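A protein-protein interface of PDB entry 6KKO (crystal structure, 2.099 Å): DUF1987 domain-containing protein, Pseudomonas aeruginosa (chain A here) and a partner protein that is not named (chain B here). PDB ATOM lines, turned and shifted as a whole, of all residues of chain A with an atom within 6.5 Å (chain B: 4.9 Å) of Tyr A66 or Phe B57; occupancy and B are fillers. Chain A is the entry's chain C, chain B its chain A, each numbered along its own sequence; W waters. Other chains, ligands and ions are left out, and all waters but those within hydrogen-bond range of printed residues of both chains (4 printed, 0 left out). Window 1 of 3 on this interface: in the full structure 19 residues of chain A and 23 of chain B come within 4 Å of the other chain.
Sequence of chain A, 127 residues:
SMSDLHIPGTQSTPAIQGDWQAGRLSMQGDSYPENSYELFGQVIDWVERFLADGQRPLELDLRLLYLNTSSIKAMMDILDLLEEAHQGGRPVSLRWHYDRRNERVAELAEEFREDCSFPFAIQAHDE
OE2 of Glu B62 sits at hydrogen-bond distance from OH of Tyr A66.
OD1 of Asp A30 sits at hydrogen-bond distance from N of Tyr A66. N of Ser A31 lies within hydrogen-bond range of O of Tyr A66, 2.8 Å away.
Phe B57 touches Tyr A32. Ile B61 touches Tyr A32 (CD1 to CE2, 3.8 Å). Tyr A66 touches Met B54 (N to CE, 3.97 Å). Tyr A66 touches Phe B57. Ala B58 touches Tyr A66. CG2 of Ile B61 touches OH of Tyr A66, at 3.6 Å.
Tyr A66 touches just these residues of chain B: Met B54, Phe B57, Ala B58, Ile B61 and Glu B62. Of the printed residues of chain B, Tyr A32 touches Phe B57 and Ile B61. Of the printed residues of chain A, Ala B58 touches Tyr A66 (3.4 Å). The nearest printed residue of chain B that does not touch Tyr A66 is Val B59 (5.5 Å). The nearest residue of chain A that does not touch Phe B57 is Asp A30 (5.6 Å). The nearest printed residue of chain A that does not touch Ala B58 is Leu A67 (6.1 Å).
Hydrophobic or aromatic side chains of chain A that line the printed part of chain B: Tyr A32 and Tyr A66. Of the 14 printed residues of chain B, 5 touch a printed residue of chain A. Printed residues of chain B that touch a printed residue of chain A: Met B54, Phe B57, Ala B58, Ile B61 and Glu B62. Hydrophobic or aromatic side chains of chain B that line the printed part of chain A: Met B54, Phe B57, Ala B58 and Ile B61. Among the printed residues, no Asp or Glu carboxylate lies within 4 Å of a Lys or Arg side-chain nitrogen of the other chain.
Water W2 lies within hydrogen-bond range of OH of Tyr A32 (2.5 Å) and NH2 of Arg B40 (3.4 Å). Water W1 lies within hydrogen-bond range of NH2 of Arg B40 (2.7 Å) and OH of Tyr A32 (2.9 Å). Water W3 bridges O1P of TPO A69 (2.8 Å) and O of Glu B62 (3.1 Å). Water W4 bridges the backbone carbonyl oxygen of Leu A67 (2.8 Å) and the side-chain carboxylate of Glu B62 (2.8 Å).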
ATOM      1  N   GLY A  29      36.794  33.837  -7.712  1.00  0.00           N
ATOM      2  CA  GLY A  29      35.391  33.815  -7.335  1.00  0.00           C
ATOM      3  C   GLY A  29      34.537  32.996  -8.293  1.00  0.00           C
ATOM      4  O   GLY A  29      35.019  32.351  -9.227  1.00  0.00           O
ATOM      5  N   ASP A  30      33.234  33.004  -8.013  1.00  0.00           N
ATOM      6  CA  ASP A  30      32.285  32.402  -8.936  1.00  0.00           C
ATOM      7  C   ASP A  30      32.058  33.333 -10.123  1.00  0.00           C
ATOM      8  O   ASP A  30      32.424  34.512 -10.103  1.00  0.00           O
ATOM      9  CB  ASP A  30      30.952  32.093  -8.254  1.00  0.00           C
ATOM     10  CG  ASP A  30      31.094  31.121  -7.086  1.00  0.00           C
ATOM     11  OD1 ASP A  30      31.537  29.972  -7.303  1.00  0.00           O
ATOM     12  OD2 ASP A  30      30.735  31.501  -5.951  1.00  0.00           O
ATOM     13  N   SER A  31      31.465  32.779 -11.179  1.00  0.00           N
ATOM     14  CA  SER A  31      31.160  33.569 -12.372  1.00  0.00           C
ATOM     15  C   SER A  31      29.886  32.996 -12.991  1.00  0.00           C
ATOM     16  O   SER A  31      29.931  32.024 -13.745  1.00  0.00           O
ATOM     17  CB  SER A  31      32.316  33.559 -13.363  1.00  0.00           C
ATOM     18  OG  SER A  31      32.000  34.322 -14.514  1.00  0.00           O
ATOM     19  N   TYR A  32      28.747  33.597 -12.651  1.00  0.00           N
ATOM     20  CA  TYR A  32      27.546  33.178 -13.364  1.00  0.00           C
ATOM     21  C   TYR A  32      26.649  34.354 -13.734  1.00  0.00           C
ATOM     22  O   TYR A  32      25.440  34.317 -13.473  1.00  0.00           O
ATOM     23  CB  TYR A  32      26.771  32.137 -12.549  1.00  0.00           C
ATOM     24  CG  TYR A  32      26.457  32.510 -11.114  1.00  0.00           C
ATOM     25  CD1 TYR A  32      27.415  32.381 -10.120  1.00  0.00           C
ATOM     26  CD2 TYR A  32      25.182  32.934 -10.742  1.00  0.00           C
ATOM     27  CE1 TYR A  32      27.134  32.697  -8.800  1.00  0.00           C
ATOM     28  CE2 TYR A  32      24.890  33.243  -9.426  1.00  0.00           C
ATOM     29  CZ  TYR A  32      25.869  33.129  -8.463  1.00  0.00           C
ATOM     30  OH  TYR A  32      25.608  33.427  -7.145  1.00  0.00           O
ATOM     31  N   LEU A  64      39.232  30.571  -9.795  1.00  0.00           N
ATOM     32  CA  LEU A  64      37.827  30.543 -10.159  1.00  0.00           C
ATOM     33  C   LEU A  64      37.163  29.283  -9.615  1.00  0.00           C
ATOM     34  O   LEU A  64      37.806  28.244  -9.437  1.00  0.00           O
ATOM     35  CB  LEU A  64      37.669  30.612 -11.681  1.00  0.00           C
ATOM     36  CG  LEU A  64      38.117  31.894 -12.391  1.00  0.00           C
ATOM     37  CD1 LEU A  64      38.223  31.675 -13.890  1.00  0.00           C
ATOM     38  CD2 LEU A  64      37.154  33.046 -12.111  1.00  0.00           C
ATOM     39  N   LEU A  65      35.886  29.400  -9.320  1.00  0.00           N
ATOM     40  CA  LEU A  65      35.096  28.334  -8.760  1.00  0.00           C
ATOM     41  C   LEU A  65      34.001  27.846  -9.692  1.00  0.00           C
ATOM     42  O   LEU A  65      34.284  27.167 -10.637  1.00  0.00           O
ATOM     43  CB  LEU A  65      34.569  28.742  -7.387  1.00  0.00           C
ATOM     44  CG  LEU A  65      35.618  29.352  -6.461  1.00  0.00           C
ATOM     45  CD1 LEU A  65      35.037  30.203  -5.363  1.00  0.00           C
ATOM     46  CD2 LEU A  65      36.486  28.289  -5.888  1.00  0.00           C
ATOM     47  N   TYR A  66      32.764  28.199  -9.439  1.00  0.00           N
ATOM     48  CA  TYR A  66      31.694  27.787 -10.336  1.00  0.00           C
ATOM     49  C   TYR A  66      31.569  28.771 -11.493  1.00  0.00           C
ATOM     50  O   TYR A  66      31.387  29.976 -11.280  1.00  0.00           O
ATOM     51  CB  TYR A  66      30.353  27.669  -9.611  1.00  0.00           C
ATOM     52  CG  TYR A  66      29.193  27.610 -10.586  1.00  0.00           C
ATOM     53  CD1 TYR A  66      29.092  26.569 -11.497  1.00  0.00           C
ATOM     54  CD2 TYR A  66      28.208  28.599 -10.602  1.00  0.00           C
ATOM     55  CE1 TYR A  66      28.057  26.507 -12.398  1.00  0.00           C
ATOM     56  CE2 TYR A  66      27.157  28.541 -11.498  1.00  0.00           C
ATOM     57  CZ  TYR A  66      27.087  27.487 -12.397  1.00  0.00           C
ATOM     58  OH  TYR A  66      26.057  27.402 -13.309  1.00  0.00           O
ATOM     59  N   LEU A  67      31.638  28.247 -12.715  1.00  0.00           N
ATOM     60  CA  LEU A  67      31.425  29.019 -13.931  1.00  0.00           C
ATOM     61  C   LEU A  67      30.196  28.466 -14.629  1.00  0.00           C
ATOM     62  O   LEU A  67      30.077  27.246 -14.797  1.00  0.00           O
ATOM     63  CB  LEU A  67      32.629  28.938 -14.875  1.00  0.00           C
ATOM     64  CG  LEU A  67      33.826  29.860 -14.641  1.00  0.00           C
ATOM     65  CD1 LEU A  67      34.463  29.600 -13.279  1.00  0.00           C
ATOM     66  CD2 LEU A  67      34.830  29.662 -15.766  1.00  0.00           C
ATOM     67  N   ASN A  68      29.296  29.354 -15.053  1.00  0.00           N
ATOM     68  CA  ASN A  68      28.137  28.916 -15.825  1.00  0.00           C
ATOM     69  C   ASN A  68      28.556  28.755 -17.291  1.00  0.00           C
ATOM     70  O   ASN A  68      29.714  28.987 -17.626  1.00  0.00           O
ATOM     71  CB  ASN A  68      26.956  29.902 -15.660  1.00  0.00           C
ATOM     72  CG  ASN A  68      27.219  31.272 -16.288  1.00  0.00           C
ATOM     73  OD1 ASN A  68      28.349  31.633 -16.607  1.00  0.00           O
ATOM     74  ND2 ASN A  68      26.150  32.051 -16.447  1.00  0.00           N
ATOM     75  N   TPO A  69      27.626  28.340 -18.153  1.00  0.00           N
ATOM     76  CA  TPO A  69      27.946  28.011 -19.546  1.00  0.00           C
ATOM     77  CB  TPO A  69      26.688  27.440 -20.203  1.00  0.00           C
ATOM     78  CG2 TPO A  69      26.353  26.059 -19.651  1.00  0.00           C
ATOM     79  OG1 TPO A  69      25.598  28.338 -19.989  1.00  0.00           O
ATOM     80  P   TPO A  69      24.714  28.453 -21.338  1.00  0.00           P
ATOM     81  O1P TPO A  69      23.484  27.603 -21.134  1.00  0.00           O
ATOM     82  O2P TPO A  69      24.333  29.906 -21.513  1.00  0.00           O
ATOM     83  O3P TPO A  69      25.535  27.962 -22.509  1.00  0.00           O
ATOM     84  C   TPO A  69      28.468  29.190 -20.332  1.00  0.00           C
ATOM     85  O   TPO A  69      29.401  29.051 -21.163  1.00  0.00           O
ATOM     86  N   SER A  71      30.065  31.852 -19.100  1.00  0.00           N
ATOM     87  CA  SER A  71      31.425  32.148 -18.663  1.00  0.00           C
ATOM     88  C   SER A  71      32.422  31.139 -19.217  1.00  0.00           C
ATOM     89  O   SER A  71      33.586  31.489 -19.449  1.00  0.00           O
ATOM     90  CB  SER A  71      31.495  32.188 -17.136  1.00  0.00           C
ATOM     91  OG  SER A  71      30.604  33.166 -16.618  1.00  0.00           O
ATOM     92  N   VAL A 105      36.232  21.678  -9.611  1.00  0.00           N
ATOM     93  CA  VAL A 105      37.016  22.781 -10.152  1.00  0.00           C
ATOM     94  C   VAL A 105      38.249  22.256 -10.879  1.00  0.00           C
ATOM     95  O   VAL A 105      38.642  22.782 -11.927  1.00  0.00           O
ATOM     96  CB  VAL A 105      37.381  23.763  -9.030  1.00  0.00           C
ATOM     97  CG1 VAL A 105      38.279  24.847  -9.565  1.00  0.00           C
ATOM     98  CG2 VAL A 105      36.102  24.371  -8.438  1.00  0.00           C
ATOM     99  N   LEU A 108      37.016  20.825 -14.193  1.00  0.00           N
ATOM    100  CA  LEU A 108      36.746  21.873 -15.174  1.00  0.00           C
ATOM    101  C   LEU A 108      38.042  22.436 -15.745  1.00  0.00           C
ATOM    102  O   LEU A 108      38.183  22.587 -16.966  1.00  0.00           O
ATOM    103  CB  LEU A 108      35.924  22.994 -14.534  1.00  0.00           C
ATOM    104  CG  LEU A 108      35.730  24.213 -15.440  1.00  0.00           C
ATOM    105  CD1 LEU A 108      34.946  23.834 -16.690  1.00  0.00           C
ATOM    106  CD2 LEU A 108      35.049  25.343 -14.697  1.00  0.00           C
ATOM    107  N   GLY B  36      19.360  31.123  -5.148  1.00  0.00           N
ATOM    108  CA  GLY B  36      20.593  30.342  -5.143  1.00  0.00           C
ATOM    109  C   GLY B  36      21.358  30.486  -3.843  1.00  0.00           C
ATOM    110  O   GLY B  36      22.072  29.570  -3.432  1.00  0.00           O
ATOM    111  N   LEU B  39      19.648  28.242  -1.436  1.00  0.00           N
ATOM    112  CA  LEU B  39      20.031  26.874  -1.781  1.00  0.00           C
ATOM    113  C   LEU B  39      21.423  26.540  -1.261  1.00  0.00           C
ATOM    114  O   LEU B  39      21.647  25.461  -0.698  1.00  0.00           O
ATOM    115  CB  LEU B  39      19.957  26.685  -3.294  1.00  0.00           C
ATOM    116  CG  LEU B  39      20.473  25.354  -3.838  1.00  0.00           C
ATOM    117  CD1 LEU B  39      19.717  24.146  -3.265  1.00  0.00           C
ATOM    118  CD2 LEU B  39      20.415  25.381  -5.357  1.00  0.00           C
ATOM    119  N   ARG B  40      22.378  27.454  -1.460  1.00  0.00           N
ATOM    120  CA  ARG B  40      23.746  27.217  -1.012  1.00  0.00           C
ATOM    121  C   ARG B  40      23.819  27.128   0.506  1.00  0.00           C
ATOM    122  O   ARG B  40      24.575  26.320   1.050  1.00  0.00           O
ATOM    123  CB  ARG B  40      24.670  28.320  -1.531  1.00  0.00           C
ATOM    124  CG  ARG B  40      24.949  28.219  -3.026  1.00  0.00           C
ATOM    125  CD  ARG B  40      25.912  29.289  -3.524  1.00  0.00           C
ATOM    126  NE  ARG B  40      25.290  30.601  -3.690  1.00  0.00           N
ATOM    127  CZ  ARG B  40      25.502  31.631  -2.878  1.00  0.00           C
ATOM    128  NH1 ARG B  40      26.322  31.501  -1.843  1.00  0.00           N
ATOM    129  NH2 ARG B  40      24.904  32.792  -3.100  1.00  0.00           N
ATOM    130  N   LEU B  43      22.410  23.667   1.407  1.00  0.00           N
ATOM    131  CA  LEU B  43      23.390  22.622   1.128  1.00  0.00           C
ATOM    132  C   LEU B  43      24.495  22.602   2.179  1.00  0.00           C
ATOM    133  O   LEU B  43      24.971  21.528   2.568  1.00  0.00           O
ATOM    134  CB  LEU B  43      23.984  22.810  -0.270  1.00  0.00           C
ATOM    135  CG  LEU B  43      23.038  22.567  -1.450  1.00  0.00           C
ATOM    136  CD1 LEU B  43      23.591  23.168  -2.732  1.00  0.00           C
ATOM    137  CD2 LEU B  43      22.816  21.068  -1.605  1.00  0.00           C
ATOM    138  N   ALA B  53      27.585  19.891  -3.620  1.00  0.00           N
ATOM    139  CA  ALA B  53      26.987  21.212  -3.458  1.00  0.00           C
ATOM    140  C   ALA B  53      27.129  22.046  -4.723  1.00  0.00           C
ATOM    141  O   ALA B  53      26.238  22.834  -5.058  1.00  0.00           O
ATOM    142  CB  ALA B  53      27.613  21.942  -2.269  1.00  0.00           C
ATOM    143  N   MET B  54      28.234  21.889  -5.443  1.00  0.00           N
ATOM    144  CA  MET B  54      28.423  22.686  -6.639  1.00  0.00           C
ATOM    145  C   MET B  54      27.547  22.166  -7.772  1.00  0.00           C
ATOM    146  O   MET B  54      27.001  22.945  -8.549  1.00  0.00           O
ATOM    147  CB  MET B  54      29.884  22.708  -7.065  1.00  0.00           C
ATOM    148  CG  MET B  54      30.134  23.644  -8.233  1.00  0.00           C
ATOM    149  SD  MET B  54      32.011  24.090  -8.457  1.00  0.00           S
ATOM    150  CE  MET B  54      32.277  25.208  -6.877  1.00  0.00           C
ATOM    151  N   ASP B  55      27.405  20.840  -7.840  1.00  0.00           N
ATOM    152  CA  ASP B  55      26.563  20.234  -8.867  1.00  0.00           C
ATOM    153  C   ASP B  55      25.114  20.695  -8.734  1.00  0.00           C
ATOM    154  O   ASP B  55      24.487  21.095  -9.720  1.00  0.00           O
ATOM    155  CB  ASP B  55      26.649  18.708  -8.784  1.00  0.00           C
ATOM    156  CG  ASP B  55      27.945  18.157  -9.369  1.00  0.00           C
ATOM    157  OD1 ASP B  55      28.658  18.905 -10.070  1.00  0.00           O
ATOM    158  OD2 ASP B  55      28.255  16.974  -9.113  1.00  0.00           O
ATOM    159  N   VAL B  56      24.561  20.638  -7.520  1.00  0.00           N
ATOM    160  CA  VAL B  56      23.175  21.054  -7.307  1.00  0.00           C
ATOM    161  C   VAL B  56      23.005  22.538  -7.626  1.00  0.00           C
ATOM    162  O   VAL B  56      22.033  22.944  -8.276  1.00  0.00           O
ATOM    163  CB  VAL B  56      22.725  20.731  -5.870  1.00  0.00           C
ATOM    164  CG1 VAL B  56      21.293  21.206  -5.652  1.00  0.00           C
ATOM    165  CG2 VAL B  56      22.852  19.232  -5.584  1.00  0.00           C
ATOM    166  N   PHE B  57      23.936  23.372  -7.152  1.00  0.00           N
ATOM    167  CA  PHE B  57      23.873  24.799  -7.458  1.00  0.00           C
ATOM    168  C   PHE B  57      24.007  25.041  -8.959  1.00  0.00           C
ATOM    169  O   PHE B  57      23.233  25.808  -9.545  1.00  0.00           O
ATOM    170  CB  PHE B  57      24.954  25.553  -6.679  1.00  0.00           C
ATOM    171  CG  PHE B  57      24.956  27.037  -6.919  1.00  0.00           C
ATOM    172  CD1 PHE B  57      23.968  27.849  -6.381  1.00  0.00           C
ATOM    173  CD2 PHE B  57      25.956  27.626  -7.682  1.00  0.00           C
ATOM    174  CE1 PHE B  57      23.970  29.218  -6.602  1.00  0.00           C
ATOM    175  CE2 PHE B  57      25.965  28.992  -7.905  1.00  0.00           C
ATOM    176  CZ  PHE B  57      24.973  29.788  -7.364  1.00  0.00           C
ATOM    177  N   ALA B  58      24.969  24.370  -9.602  1.00  0.00           N
ATOM    178  CA  ALA B  58      25.173  24.551 -11.037  1.00  0.00           C
ATOM    179  C   ALA B  58      23.936  24.160 -11.833  1.00  0.00           C
ATOM    180  O   ALA B  58      23.572  24.847 -12.791  1.00  0.00           O
ATOM    181  CB  ALA B  58      26.374  23.734 -11.510  1.00  0.00           C
ATOM    182  N   VAL B  59      23.269  23.069 -11.449  1.00  0.00           N
ATOM    183  CA  VAL B  59      22.080  22.644 -12.186  1.00  0.00           C
ATOM    184  C   VAL B  59      20.936  23.633 -11.966  1.00  0.00           C
ATOM    185  O   VAL B  59      20.153  23.914 -12.885  1.00  0.00           O
ATOM    186  CB  VAL B  59      21.690  21.206 -11.791  1.00  0.00           C
ATOM    187  CG1 VAL B  59      20.275  20.895 -12.229  1.00  0.00           C
ATOM    188  CG2 VAL B  59      22.663  20.193 -12.422  1.00  0.00           C
ATOM    189  N   TYR B  60      20.823  24.176 -10.746  1.00  0.00           N
ATOM    190  CA  TYR B  60      19.806  25.187 -10.463  1.00  0.00           C
ATOM    191  C   TYR B  60      20.026  26.437 -11.306  1.00  0.00           C
ATOM    192  O   TYR B  60      19.084  26.980 -11.893  1.00  0.00           O
ATOM    193  CB  TYR B  60      19.827  25.550  -8.977  1.00  0.00           C
ATOM    194  CG  TYR B  60      19.183  26.883  -8.670  1.00  0.00           C
ATOM    195  CD1 TYR B  60      17.807  27.023  -8.603  1.00  0.00           C
ATOM    196  CD2 TYR B  60      19.967  28.023  -8.514  1.00  0.00           C
ATOM    197  CE1 TYR B  60      17.221  28.259  -8.341  1.00  0.00           C
ATOM    198  CE2 TYR B  60      19.399  29.250  -8.262  1.00  0.00           C
ATOM    199  CZ  TYR B  60      18.030  29.368  -8.175  1.00  0.00           C
ATOM    200  OH  TYR B  60      17.486  30.608  -7.925  1.00  0.00           O
ATOM    201  N   ILE B  61      21.263  26.942 -11.329  1.00  0.00           N
ATOM    202  CA  ILE B  61      21.550  28.172 -12.057  1.00  0.00           C
ATOM    203  C   ILE B  61      21.323  27.966 -13.545  1.00  0.00           C
ATOM    204  O   ILE B  61      20.702  28.798 -14.217  1.00  0.00           O
ATOM    205  CB  ILE B  61      22.988  28.646 -11.767  1.00  0.00           C
ATOM    206  CG1 ILE B  61      23.115  29.155 -10.323  1.00  0.00           C
ATOM    207  CG2 ILE B  61      23.413  29.715 -12.773  1.00  0.00           C
ATOM    208  CD1 ILE B  61      22.386  30.450 -10.036  1.00  0.00           C
ATOM    209  N   GLU B  62      21.801  26.845 -14.081  1.00  0.00           N
ATOM    210  CA  GLU B  62      21.724  26.668 -15.525  1.00  0.00           C
ATOM    211  C   GLU B  62      20.286  26.450 -15.988  1.00  0.00           C
ATOM    212  O   GLU B  62      19.891  26.970 -17.037  1.00  0.00           O
ATOM    213  CB  GLU B  62      22.659  25.534 -15.950  1.00  0.00           C
ATOM    214  CG  GLU B  62      24.121  26.010 -16.036  1.00  0.00           C
ATOM    215  CD  GLU B  62      25.129  24.926 -15.691  1.00  0.00           C
ATOM    216  OE1 GLU B  62      24.884  23.761 -16.055  1.00  0.00           O
ATOM    217  OE2 GLU B  62      26.162  25.244 -15.051  1.00  0.00           O
HETATM  218  O   HOH W   1      23.525  32.453  -5.383  1.00  0.00           O
HETATM  219  O   HOH W   2      27.336  33.107  -5.385  1.00  0.00           O
HETATM  220  O   HOH W   3      22.595  27.557 -18.522  1.00  0.00           O
HETATM  221  O   HOH W   4      28.866  24.920 -15.688  1.00  0.00           O
